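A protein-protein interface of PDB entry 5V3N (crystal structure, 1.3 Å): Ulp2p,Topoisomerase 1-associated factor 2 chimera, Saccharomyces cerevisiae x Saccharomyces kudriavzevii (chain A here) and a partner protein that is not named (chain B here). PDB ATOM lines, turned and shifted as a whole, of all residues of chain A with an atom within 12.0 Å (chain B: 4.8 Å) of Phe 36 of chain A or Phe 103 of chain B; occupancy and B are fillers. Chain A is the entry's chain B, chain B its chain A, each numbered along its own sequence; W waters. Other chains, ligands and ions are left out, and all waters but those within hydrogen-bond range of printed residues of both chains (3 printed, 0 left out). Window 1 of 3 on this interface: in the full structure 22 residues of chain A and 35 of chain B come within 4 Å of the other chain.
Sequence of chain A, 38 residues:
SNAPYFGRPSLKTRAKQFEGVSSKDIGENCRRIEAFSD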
ATOM      1  N   CYS A  30      -0.171 -17.194 -23.291  1.00  0.00           N
ATOM      2  CA  CYS A  30      -0.387 -18.535 -22.782  1.00  0.00           C
ATOM      3  C   CYS A  30      -0.435 -19.488 -23.985  1.00  0.00           C
ATOM      4  O   CYS A  30      -0.916 -19.131 -25.061  1.00  0.00           O
ATOM      5  CB  CYS A  30      -1.726 -18.689 -21.997  1.00  0.00           C
ATOM      6  SG  CYS A  30      -2.055 -17.575 -20.710  1.00  0.00           S
ATOM      7  N   ARG A  31       0.125 -20.664 -23.818  1.00  0.00           N
ATOM      8  CA  ARG A  31      -0.002 -21.766 -24.802  1.00  0.00           C
ATOM      9  C   ARG A  31      -1.301 -22.484 -24.457  1.00  0.00           C
ATOM     10  O   ARG A  31      -1.518 -22.882 -23.303  1.00  0.00           O
ATOM     11  CB  ARG A  31       1.205 -22.651 -24.626  1.00  0.00           C
ATOM     12  CG  ARG A  31       1.140 -24.006 -25.312  1.00  0.00           C
ATOM     13  CD  ARG A  31       2.385 -24.762 -25.058  1.00  0.00           C
ATOM     14  NE  ARG A  31       2.386 -26.074 -25.691  1.00  0.00           N
ATOM     15  CZ  ARG A  31       3.421 -26.905 -25.597  1.00  0.00           C
ATOM     16  NH1 ARG A  31       4.533 -26.561 -24.926  1.00  0.00           N
ATOM     17  NH2 ARG A  31       3.344 -28.106 -26.150  1.00  0.00           N
ATOM     18  N   ARG A  32      -2.207 -22.579 -25.429  1.00  0.00           N
ATOM     19  CA  ARG A  32      -3.535 -23.100 -25.191  1.00  0.00           C
ATOM     20  C   ARG A  32      -3.534 -24.596 -25.477  1.00  0.00           C
ATOM     21  O   ARG A  32      -3.170 -25.027 -26.586  1.00  0.00           O
ATOM     22  CB  ARG A  32      -4.561 -22.410 -26.092  1.00  0.00           C
ATOM     23  CG  ARG A  32      -5.935 -22.980 -25.966  1.00  0.00           C
ATOM     24  CD  ARG A  32      -6.694 -22.648 -24.655  1.00  0.00           C
ATOM     25  NE  ARG A  32      -8.115 -23.013 -24.746  1.00  0.00           N
ATOM     26  CZ  ARG A  32      -8.986 -22.703 -23.774  1.00  0.00           C
ATOM     27  NH1 ARG A  32      -8.510 -22.120 -22.718  1.00  0.00           N
ATOM     28  NH2 ARG A  32     -10.300 -23.030 -23.817  1.00  0.00           N
ATOM     29  N   ILE A  33      -3.962 -25.395 -24.511  1.00  0.00           N
ATOM     30  CA  ILE A  33      -4.093 -26.849 -24.605  1.00  0.00           C
ATOM     31  C   ILE A  33      -5.525 -27.264 -24.259  1.00  0.00           C
ATOM     32  O   ILE A  33      -6.070 -26.818 -23.238  1.00  0.00           O
ATOM     33  CB  ILE A  33      -3.057 -27.566 -23.742  1.00  0.00           C
ATOM     34  CG1 ILE A  33      -1.632 -27.143 -24.226  1.00  0.00           C
ATOM     35  CG2 ILE A  33      -3.248 -29.144 -23.851  1.00  0.00           C
ATOM     36  CD1 ILE A  33      -0.455 -27.826 -23.529  1.00  0.00           C
ATOM     37  N   GLU A  34      -6.169 -28.098 -25.092  1.00  0.00           N
ATOM     38  CA  GLU A  34      -7.579 -28.423 -24.837  1.00  0.00           C
ATOM     39  C   GLU A  34      -7.760 -29.562 -23.846  1.00  0.00           C
ATOM     40  O   GLU A  34      -8.797 -29.635 -23.185  1.00  0.00           O
ATOM     41  CB  GLU A  34      -8.260 -28.817 -26.159  1.00  0.00           C
ATOM     42  CG  GLU A  34      -8.104 -27.752 -27.251  1.00  0.00           C
ATOM     43  CD  GLU A  34      -8.417 -26.348 -26.890  1.00  0.00           C
ATOM     44  OE1 GLU A  34      -9.386 -26.133 -26.162  1.00  0.00           O
ATOM     45  OE2 GLU A  34      -7.669 -25.446 -27.393  1.00  0.00           O
ATOM     46  N   ALA A  35      -6.808 -30.472 -23.673  1.00  0.00           N
ATOM     47  CA  ALA A  35      -7.067 -31.626 -22.808  1.00  0.00           C
ATOM     48  C   ALA A  35      -5.723 -32.282 -22.514  1.00  0.00           C
ATOM     49  O   ALA A  35      -4.717 -31.954 -23.198  1.00  0.00           O
ATOM     50  CB  ALA A  35      -7.994 -32.659 -23.548  1.00  0.00           C
ATOM     51  N   PHE A  36      -5.700 -33.119 -21.460  1.00  0.00           N
ATOM     52  CA  PHE A  36      -4.463 -33.761 -21.059  1.00  0.00           C
ATOM     53  C   PHE A  36      -4.772 -35.236 -20.951  1.00  0.00           C
ATOM     54  O   PHE A  36      -5.828 -35.610 -20.429  1.00  0.00           O
ATOM     55  CB  PHE A  36      -3.949 -33.207 -19.725  1.00  0.00           C
ATOM     56  CG  PHE A  36      -3.828 -31.754 -19.769  1.00  0.00           C
ATOM     57  CD1 PHE A  36      -4.922 -30.932 -19.418  1.00  0.00           C
ATOM     58  CD2 PHE A  36      -2.647 -31.158 -20.149  1.00  0.00           C
ATOM     59  CE1 PHE A  36      -4.788 -29.566 -19.528  1.00  0.00           C
ATOM     60  CE2 PHE A  36      -2.480 -29.828 -20.266  1.00  0.00           C
ATOM     61  CZ  PHE A  36      -3.597 -28.982 -19.931  1.00  0.00           C
ATOM     62  N   SER A  37      -3.909 -36.071 -21.547  1.00  0.00           N
ATOM     63  CA  SER A  37      -4.113 -37.501 -21.534  1.00  0.00           C
ATOM     64  C   SER A  37      -3.780 -38.147 -20.191  1.00  0.00           C
ATOM     65  O   SER A  37      -3.221 -37.535 -19.276  1.00  0.00           O
ATOM     66  CB  SER A  37      -3.209 -38.171 -22.569  1.00  0.00           C
ATOM     67  OG  SER A  37      -1.839 -37.947 -22.178  1.00  0.00           O
ATOM     68  N   ASP A  38      -4.143 -39.422 -20.077  1.00  0.00           N
ATOM     69  CA  ASP A  38      -3.865 -40.200 -18.875  1.00  0.00           C
ATOM     70  C   ASP A  38      -2.747 -41.221 -19.119  1.00  0.00           C
ATOM     71  O   ASP A  38      -1.846 -40.990 -19.939  1.00  0.00           O
ATOM     72  CB  ASP A  38      -5.131 -40.919 -18.404  1.00  0.00           C
ATOM     73  CG  ASP A  38      -4.854 -41.938 -17.275  1.00  0.00           C
ATOM     74  OD1 ASP A  38      -3.693 -42.042 -16.777  1.00  0.00           O
ATOM     75  OD2 ASP A  38      -5.813 -42.635 -16.877  1.00  0.00           O
ATOM     76  N   TYR B  66      -2.534 -21.672 -15.978  1.00  0.00           N
ATOM     77  CA  TYR B  66      -1.487 -22.296 -15.192  1.00  0.00           C
ATOM     78  C   TYR B  66      -0.201 -21.526 -15.376  1.00  0.00           C
ATOM     79  O   TYR B  66       0.245 -21.361 -16.508  1.00  0.00           O
ATOM     80  CB  TYR B  66      -1.327 -23.783 -15.620  1.00  0.00           C
ATOM     81  CG  TYR B  66      -0.036 -24.426 -15.248  1.00  0.00           C
ATOM     82  CD1 TYR B  66       0.159 -25.012 -14.006  1.00  0.00           C
ATOM     83  CD2 TYR B  66       1.030 -24.519 -16.172  1.00  0.00           C
ATOM     84  CE1 TYR B  66       1.331 -25.737 -13.702  1.00  0.00           C
ATOM     85  CE2 TYR B  66       2.204 -25.171 -15.854  1.00  0.00           C
ATOM     86  CZ  TYR B  66       2.377 -25.798 -14.622  1.00  0.00           C
ATOM     87  OH  TYR B  66       3.506 -26.480 -14.316  1.00  0.00           O
ATOM     88  N   TYR B  88       5.280 -29.219 -21.656  1.00  0.00           N
ATOM     89  CA  TYR B  88       4.383 -28.083 -21.618  1.00  0.00           C
ATOM     90  C   TYR B  88       4.209 -27.540 -20.207  1.00  0.00           C
ATOM     91  O   TYR B  88       3.741 -26.399 -20.042  1.00  0.00           O
ATOM     92  CB  TYR B  88       3.077 -28.441 -22.338  1.00  0.00           C
ATOM     93  CG  TYR B  88       2.355 -29.682 -21.888  1.00  0.00           C
ATOM     94  CD1 TYR B  88       1.718 -29.768 -20.679  1.00  0.00           C
ATOM     95  CD2 TYR B  88       2.419 -30.863 -22.646  1.00  0.00           C
ATOM     96  CE1 TYR B  88       1.066 -30.837 -20.286  1.00  0.00           C
ATOM     97  CE2 TYR B  88       1.763 -31.972 -22.257  1.00  0.00           C
ATOM     98  CZ  TYR B  88       1.134 -32.026 -21.058  1.00  0.00           C
ATOM     99  OH  TYR B  88       0.454 -33.130 -20.664  1.00  0.00           O
ATOM    100  N   LEU B  89       4.559 -28.318 -19.209  1.00  0.00           N
ATOM    101  CA  LEU B  89       4.341 -27.831 -17.834  1.00  0.00           C
ATOM    102  C   LEU B  89       5.408 -26.905 -17.380  1.00  0.00           C
ATOM    103  O   LEU B  89       5.309 -26.440 -16.225  1.00  0.00           O
ATOM    104  CB  LEU B  89       4.285 -29.012 -16.886  1.00  0.00           C
ATOM    105  CG  LEU B  89       3.012 -29.838 -17.041  1.00  0.00           C
ATOM    106  CD1 LEU B  89       3.129 -31.074 -16.091  1.00  0.00           C
ATOM    107  CD2 LEU B  89       1.744 -29.031 -16.742  1.00  0.00           C
ATOM    108  N   LEU B  93       0.232 -21.878 -19.361  1.00  0.00           N
ATOM    109  CA  LEU B  93      -0.761 -22.503 -20.195  1.00  0.00           C
ATOM    110  C   LEU B  93      -2.142 -21.966 -19.930  1.00  0.00           C
ATOM    111  O   LEU B  93      -2.403 -21.429 -18.867  1.00  0.00           O
ATOM    112  CB  LEU B  93      -0.824 -23.999 -19.882  1.00  0.00           C
ATOM    113  CG  LEU B  93       0.460 -24.778 -19.985  1.00  0.00           C
ATOM    114  CD1 LEU B  93       0.181 -26.176 -19.505  1.00  0.00           C
ATOM    115  CD2 LEU B  93       1.077 -24.769 -21.399  1.00  0.00           C
ATOM    116  N   PHE B  95      -6.242 -23.482 -20.542  1.00  0.00           N
ATOM    117  CA  PHE B  95      -7.007 -24.685 -20.843  1.00  0.00           C
ATOM    118  C   PHE B  95      -8.413 -24.551 -20.326  1.00  0.00           C
ATOM    119  O   PHE B  95      -8.697 -23.655 -19.443  1.00  0.00           O
ATOM    120  CB  PHE B  95      -6.309 -25.958 -20.341  1.00  0.00           C
ATOM    121  CG  PHE B  95      -6.020 -25.976 -18.856  1.00  0.00           C
ATOM    122  CD1 PHE B  95      -7.001 -26.442 -17.975  1.00  0.00           C
ATOM    123  CD2 PHE B  95      -4.786 -25.613 -18.403  1.00  0.00           C
ATOM    124  CE1 PHE B  95      -6.742 -26.539 -16.611  1.00  0.00           C
ATOM    125  CE2 PHE B  95      -4.484 -25.696 -16.991  1.00  0.00           C
ATOM    126  CZ  PHE B  95      -5.481 -26.164 -16.159  1.00  0.00           C
ATOM    127  N   SER B  99     -11.267 -29.305 -18.295  1.00  0.00           N
ATOM    128  CA  SER B  99     -10.086 -30.155 -18.267  1.00  0.00           C
ATOM    129  C   SER B  99      -9.294 -30.022 -16.982  1.00  0.00           C
ATOM    130  O   SER B  99      -8.188 -30.541 -16.903  1.00  0.00           O
ATOM    131  CB  SER B  99      -9.177 -29.805 -19.423  1.00  0.00           C
ATOM    132  OG  SER B  99      -9.811 -30.254 -20.630  1.00  0.00           O
ATOM    133  N   LEU B 100      -9.848 -29.394 -15.939  1.00  0.00           N
ATOM    134  CA  LEU B 100      -9.041 -29.103 -14.773  1.00  0.00           C
ATOM    135  C   LEU B 100      -8.559 -30.371 -14.069  1.00  0.00           C
ATOM    136  O   LEU B 100      -7.414 -30.446 -13.623  1.00  0.00           O
ATOM    137  CB  LEU B 100      -9.876 -28.255 -13.801  1.00  0.00           C
ATOM    138  CG  LEU B 100      -9.147 -27.800 -12.545  1.00  0.00           C
ATOM    139  CD1 LEU B 100      -7.965 -26.945 -12.874  1.00  0.00           C
ATOM    140  CD2 LEU B 100     -10.087 -27.038 -11.667  1.00  0.00           C
ATOM    141  N   ASN B 101      -9.460 -31.321 -13.852  1.00  0.00           N
ATOM    142  CA  ASN B 101      -9.070 -32.567 -13.191  1.00  0.00           C
ATOM    143  C   ASN B 101      -8.074 -33.328 -14.046  1.00  0.00           C
ATOM    144  O   ASN B 101      -7.162 -33.959 -13.513  1.00  0.00           O
ATOM    145  CB  ASN B 101     -10.254 -33.425 -12.769  1.00  0.00           C
ATOM    146  CG  ASN B 101      -9.842 -34.759 -12.180  1.00  0.00           C
ATOM    147  OD1 ASN B 101     -10.092 -35.799 -12.780  1.00  0.00           O
ATOM    148  ND2 ASN B 101      -9.335 -34.746 -10.980  1.00  0.00           N
ATOM    149  N   GLN B 102      -8.245 -33.313 -15.377  1.00  0.00           N
ATOM    150  CA  GLN B 102      -7.249 -33.990 -16.218  1.00  0.00           C
ATOM    151  C   GLN B 102      -5.869 -33.392 -16.060  1.00  0.00           C
ATOM    152  O   GLN B 102      -4.848 -34.102 -16.049  1.00  0.00           O
ATOM    153  CB  GLN B 102      -7.634 -33.876 -17.722  1.00  0.00           C
ATOM    154  CG  GLN B 102      -8.856 -34.501 -18.122  1.00  0.00           C
ATOM    155  CD  GLN B 102      -9.190 -34.101 -19.638  1.00  0.00           C
ATOM    156  OE1 GLN B 102      -8.431 -33.395 -20.325  1.00  0.00           O
ATOM    157  NE2 GLN B 102     -10.342 -34.509 -20.091  1.00  0.00           N
ATOM    158  N   PHE B 103      -5.824 -32.092 -15.890  1.00  0.00           N
ATOM    159  CA  PHE B 103      -4.584 -31.383 -15.649  1.00  0.00           C
ATOM    160  C   PHE B 103      -3.945 -31.812 -14.336  1.00  0.00           C
ATOM    161  O   PHE B 103      -2.752 -32.185 -14.264  1.00  0.00           O
ATOM    162  CB  PHE B 103      -4.887 -29.881 -15.617  1.00  0.00           C
ATOM    163  CG  PHE B 103      -3.614 -29.092 -15.705  1.00  0.00           C
ATOM    164  CD1 PHE B 103      -2.770 -29.189 -16.849  1.00  0.00           C
ATOM    165  CD2 PHE B 103      -3.174 -28.489 -14.702  1.00  0.00           C
ATOM    166  CE1 PHE B 103      -1.607 -28.455 -16.891  1.00  0.00           C
ATOM    167  CE2 PHE B 103      -1.975 -27.706 -14.727  1.00  0.00           C
ATOM    168  CZ  PHE B 103      -1.233 -27.681 -15.720  1.00  0.00           C
ATOM    169  N   TYR B 104      -4.727 -31.778 -13.253  1.00  0.00           N
ATOM    170  CA  TYR B 104      -4.232 -32.249 -11.967  1.00  0.00           C
ATOM    171  C   TYR B 104      -3.653 -33.675 -12.082  1.00  0.00           C
ATOM    172  O   TYR B 104      -2.611 -34.000 -11.509  1.00  0.00           O
ATOM    173  CB  TYR B 104      -5.409 -32.231 -10.939  1.00  0.00           C
ATOM    174  CG  TYR B 104      -5.133 -33.112  -9.740  1.00  0.00           C
ATOM    175  CD1 TYR B 104      -4.318 -32.665  -8.687  1.00  0.00           C
ATOM    176  CD2 TYR B 104      -5.641 -34.337  -9.639  1.00  0.00           C
ATOM    177  CE1 TYR B 104      -3.968 -33.510  -7.637  1.00  0.00           C
ATOM    178  CE2 TYR B 104      -5.343 -35.200  -8.618  1.00  0.00           C
ATOM    179  CZ  TYR B 104      -4.488 -34.814  -7.612  1.00  0.00           C
ATOM    180  OH  TYR B 104      -4.216 -35.720  -6.596  1.00  0.00           O
ATOM    181  N   ASN B 105      -4.413 -34.567 -12.736  1.00  0.00           N
ATOM    182  CA  ASN B 105      -3.999 -35.968 -12.823  1.00  0.00           C
ATOM    183  C   ASN B 105      -2.737 -36.100 -13.640  1.00  0.00           C
ATOM    184  O   ASN B 105      -1.914 -36.987 -13.348  1.00  0.00           O
ATOM    185  CB  ASN B 105      -5.050 -36.847 -13.485  1.00  0.00           C
ATOM    186  CG  ASN B 105      -6.324 -36.996 -12.701  1.00  0.00           C
ATOM    187  OD1 ASN B 105      -6.292 -37.062 -11.508  1.00  0.00           O
ATOM    188  ND2 ASN B 105      -7.445 -37.114 -13.386  1.00  0.00           N
ATOM    189  N   LYS B 106      -2.553 -35.255 -14.644  1.00  0.00           N
ATOM    190  CA  LYS B 106      -1.308 -35.286 -15.411  1.00  0.00           C
ATOM    191  C   LYS B 106      -0.102 -34.908 -14.585  1.00  0.00           C
ATOM    192  O   LYS B 106       0.917 -35.617 -14.574  1.00  0.00           O
ATOM    193  CB  LYS B 106      -1.453 -34.357 -16.608  1.00  0.00           C
ATOM    194  CG  LYS B 106      -0.169 -34.266 -17.487  1.00  0.00           C
ATOM    195  CD  LYS B 106       0.232 -35.527 -18.137  1.00  0.00           C
ATOM    196  CE  LYS B 106      -0.715 -35.849 -19.187  1.00  0.00           C
ATOM    197  NZ  LYS B 106      -0.338 -37.131 -19.881  1.00  0.00           N
ATOM    198  N   ILE B 107      -0.219 -33.866 -13.796  1.00  0.00           N
ATOM    199  CA  ILE B 107       0.891 -33.523 -12.921  1.00  0.00           C
ATOM    200  C   ILE B 107       1.089 -34.592 -11.868  1.00  0.00           C
ATOM    201  O   ILE B 107       2.238 -34.962 -11.549  1.00  0.00           O
ATOM    202  CB  ILE B 107       0.649 -32.139 -12.257  1.00  0.00           C
ATOM    203  CG1 ILE B 107       0.669 -31.042 -13.247  1.00  0.00           C
ATOM    204  CG2 ILE B 107       1.750 -31.930 -11.189  1.00  0.00           C
ATOM    205  CD1 ILE B 107       0.278 -29.696 -12.629  1.00  0.00           C
HETATM  206  O   HOH W   1      -2.720 -38.599 -16.039  1.00  0.00           O
HETATM  207  O   HOH W   2      -0.409 -38.957 -17.571  1.00  0.00           O
HETATM  208  O   HOH W   3      -4.656 -36.632 -17.131  1.00  0.00           O
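OG of Ser 99 of chain B is in hydrogen-bond range of O of Glu 34 of chain A (2.8 Å).
OE1 of Gln 102 of chain B lies within hydrogen-bond range of N of Phe 36 of chain A, 3.0 Å away.
The side-chain hydroxyl (OG) of Ser 37 of chain A sits at hydrogen-bond distance from the side-chain amino group (NZ) of Lys 106 of chain B (2.9 Å).
N of Phe 95 of chain B lies close to NH1 of Arg 32 of chain A (3.4 Å).
The backbone carbonyl oxygen (O) of Tyr 66 of chain B is in hydrogen-bond range of the backbone NH (N) of Leu 93 of chain B (2.9 Å).
The side-chain amide oxygen of Gln 102 of chain B sits at hydrogen-bond distance from the side-chain hydroxyl of Ser 99 of chain B (3.4 Å).
The guanidinium group (NE) of Arg 32 of chain A is in salt-bridge range of the side-chain carboxylate (OE2) of Glu 34 of chain A (3.6 Å).
C of Leu 93 of chain B touches CB of Cys 30 of chain A, 3.9 Å away.
Arg 31 of chain A touches Tyr 88 of chain B (NH1 to CB, 3.5 Å).
Leu 93 of chain B touches Arg 31 of chain A.
Tyr 88 of chain B touches Ile 33 of chain A (CG to CD1, 3.7 Å).
Phe 95 of chain B touches Ile 33 of chain A (CB to O, 3.0 Å).
Ala 35 of chain A touches Ser 99 of chain B (CA to OG, 3.8 Å).
Ala 35 of chain A touches Gln 102 of chain B (CB to OE1, 3.3 Å).
Phe 36 of chain A touches Tyr 88 of chain B (CE2 to CE1, 3.7 Å).
Phe 36 of chain A touches Phe 95 of chain B.
CZ of Phe 36 of chain A touches CD1 of Phe 103 of chain B, at 3.2 Å.
Of the printed residues of chain B, Arg 31 of chain A touches Tyr 88 and Leu 93.
Of the printed residues of chain B, Arg 32 of chain A touches Phe 95 (3.4 Å).
Of the printed residues of chain B, Ile 33 of chain A touches Tyr 88 (3.7 Å) and Phe 95 (3.0 Å).
Printed residues of chain B within 4 Å of Ala 35 of chain A: Ser 99 and Gln 102.
Phe 36 of chain A touches just these residues of chain B: Tyr 88 (3.7 Å), Phe 95 (3.9 Å), Gln 102 (3.0 Å) and Phe 103 (3.2 Å).
Printed residues of chain B within 4 Å of Ser 37 of chain A: Lys 106.
No residue of chain A comes within 4 Å of Tyr 66 of chain B.
Leu 93 of chain B touches two residues of chain A.
Phe 95 of chain B touches three residues of chain A.
Of chain A, only Glu 34 (2.8 Å) and Ala 35 (3.8 Å) come within 4 Å of Ser 99 of chain B.
No residue of chain A comes within 4 Å of Leu 100 of chain B.
Asn 101 of chain B touches none of the printed residues of chain A.
Gln 102 of chain B touches just these residues of chain A: Ala 35 (3.3 Å) and Phe 36 (3.0 Å).
Lys 106 of chain B touches one residue of chain A.
No residue of chain A comes within 4 Å of Ile 107 of chain B.
The nearest printed residue of chain B that does not touch Phe 36 of chain A is Ser 99 of chain B (4.1 Å).
The nearest residue of chain A that does not touch Phe 103 of chain B is Ala 35 of chain A (6.6 Å).
Of the 14 printed residues of chain B, 7 touch a printed residue of chain A.
Hydrophobic or aromatic side chains of chain B within 4 Å of the printed part of chain A: Tyr 88, Leu 93, Phe 95 and Phe 103.
Of the 9 printed residues of chain A, 8 touch a printed residue of chain B.
Among the printed residues, no Asp or Glu carboxylate lies within 4 Å of a Lys or Arg side-chain nitrogen of the other chain.
Water W3 lies within hydrogen-bond range of O of Ser 37 of chain A (2.7 Å) and O of Gln 102 of chain B (2.8 Å).
Water W2 lies within hydrogen-bond range of the side-chain amino group (NZ) of Lys 106 of chain B (2.9 Å) and the backbone carbonyl oxygen (O) of Asp 38 of chain A (3.4 Å).
Water W1 lies within hydrogen-bond range of the backbone carbonyl oxygen of Asn 105 of chain B (3.2 Å) and the backbone carbonyl oxygen of Ser 37 of chain A (3.4 Å).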
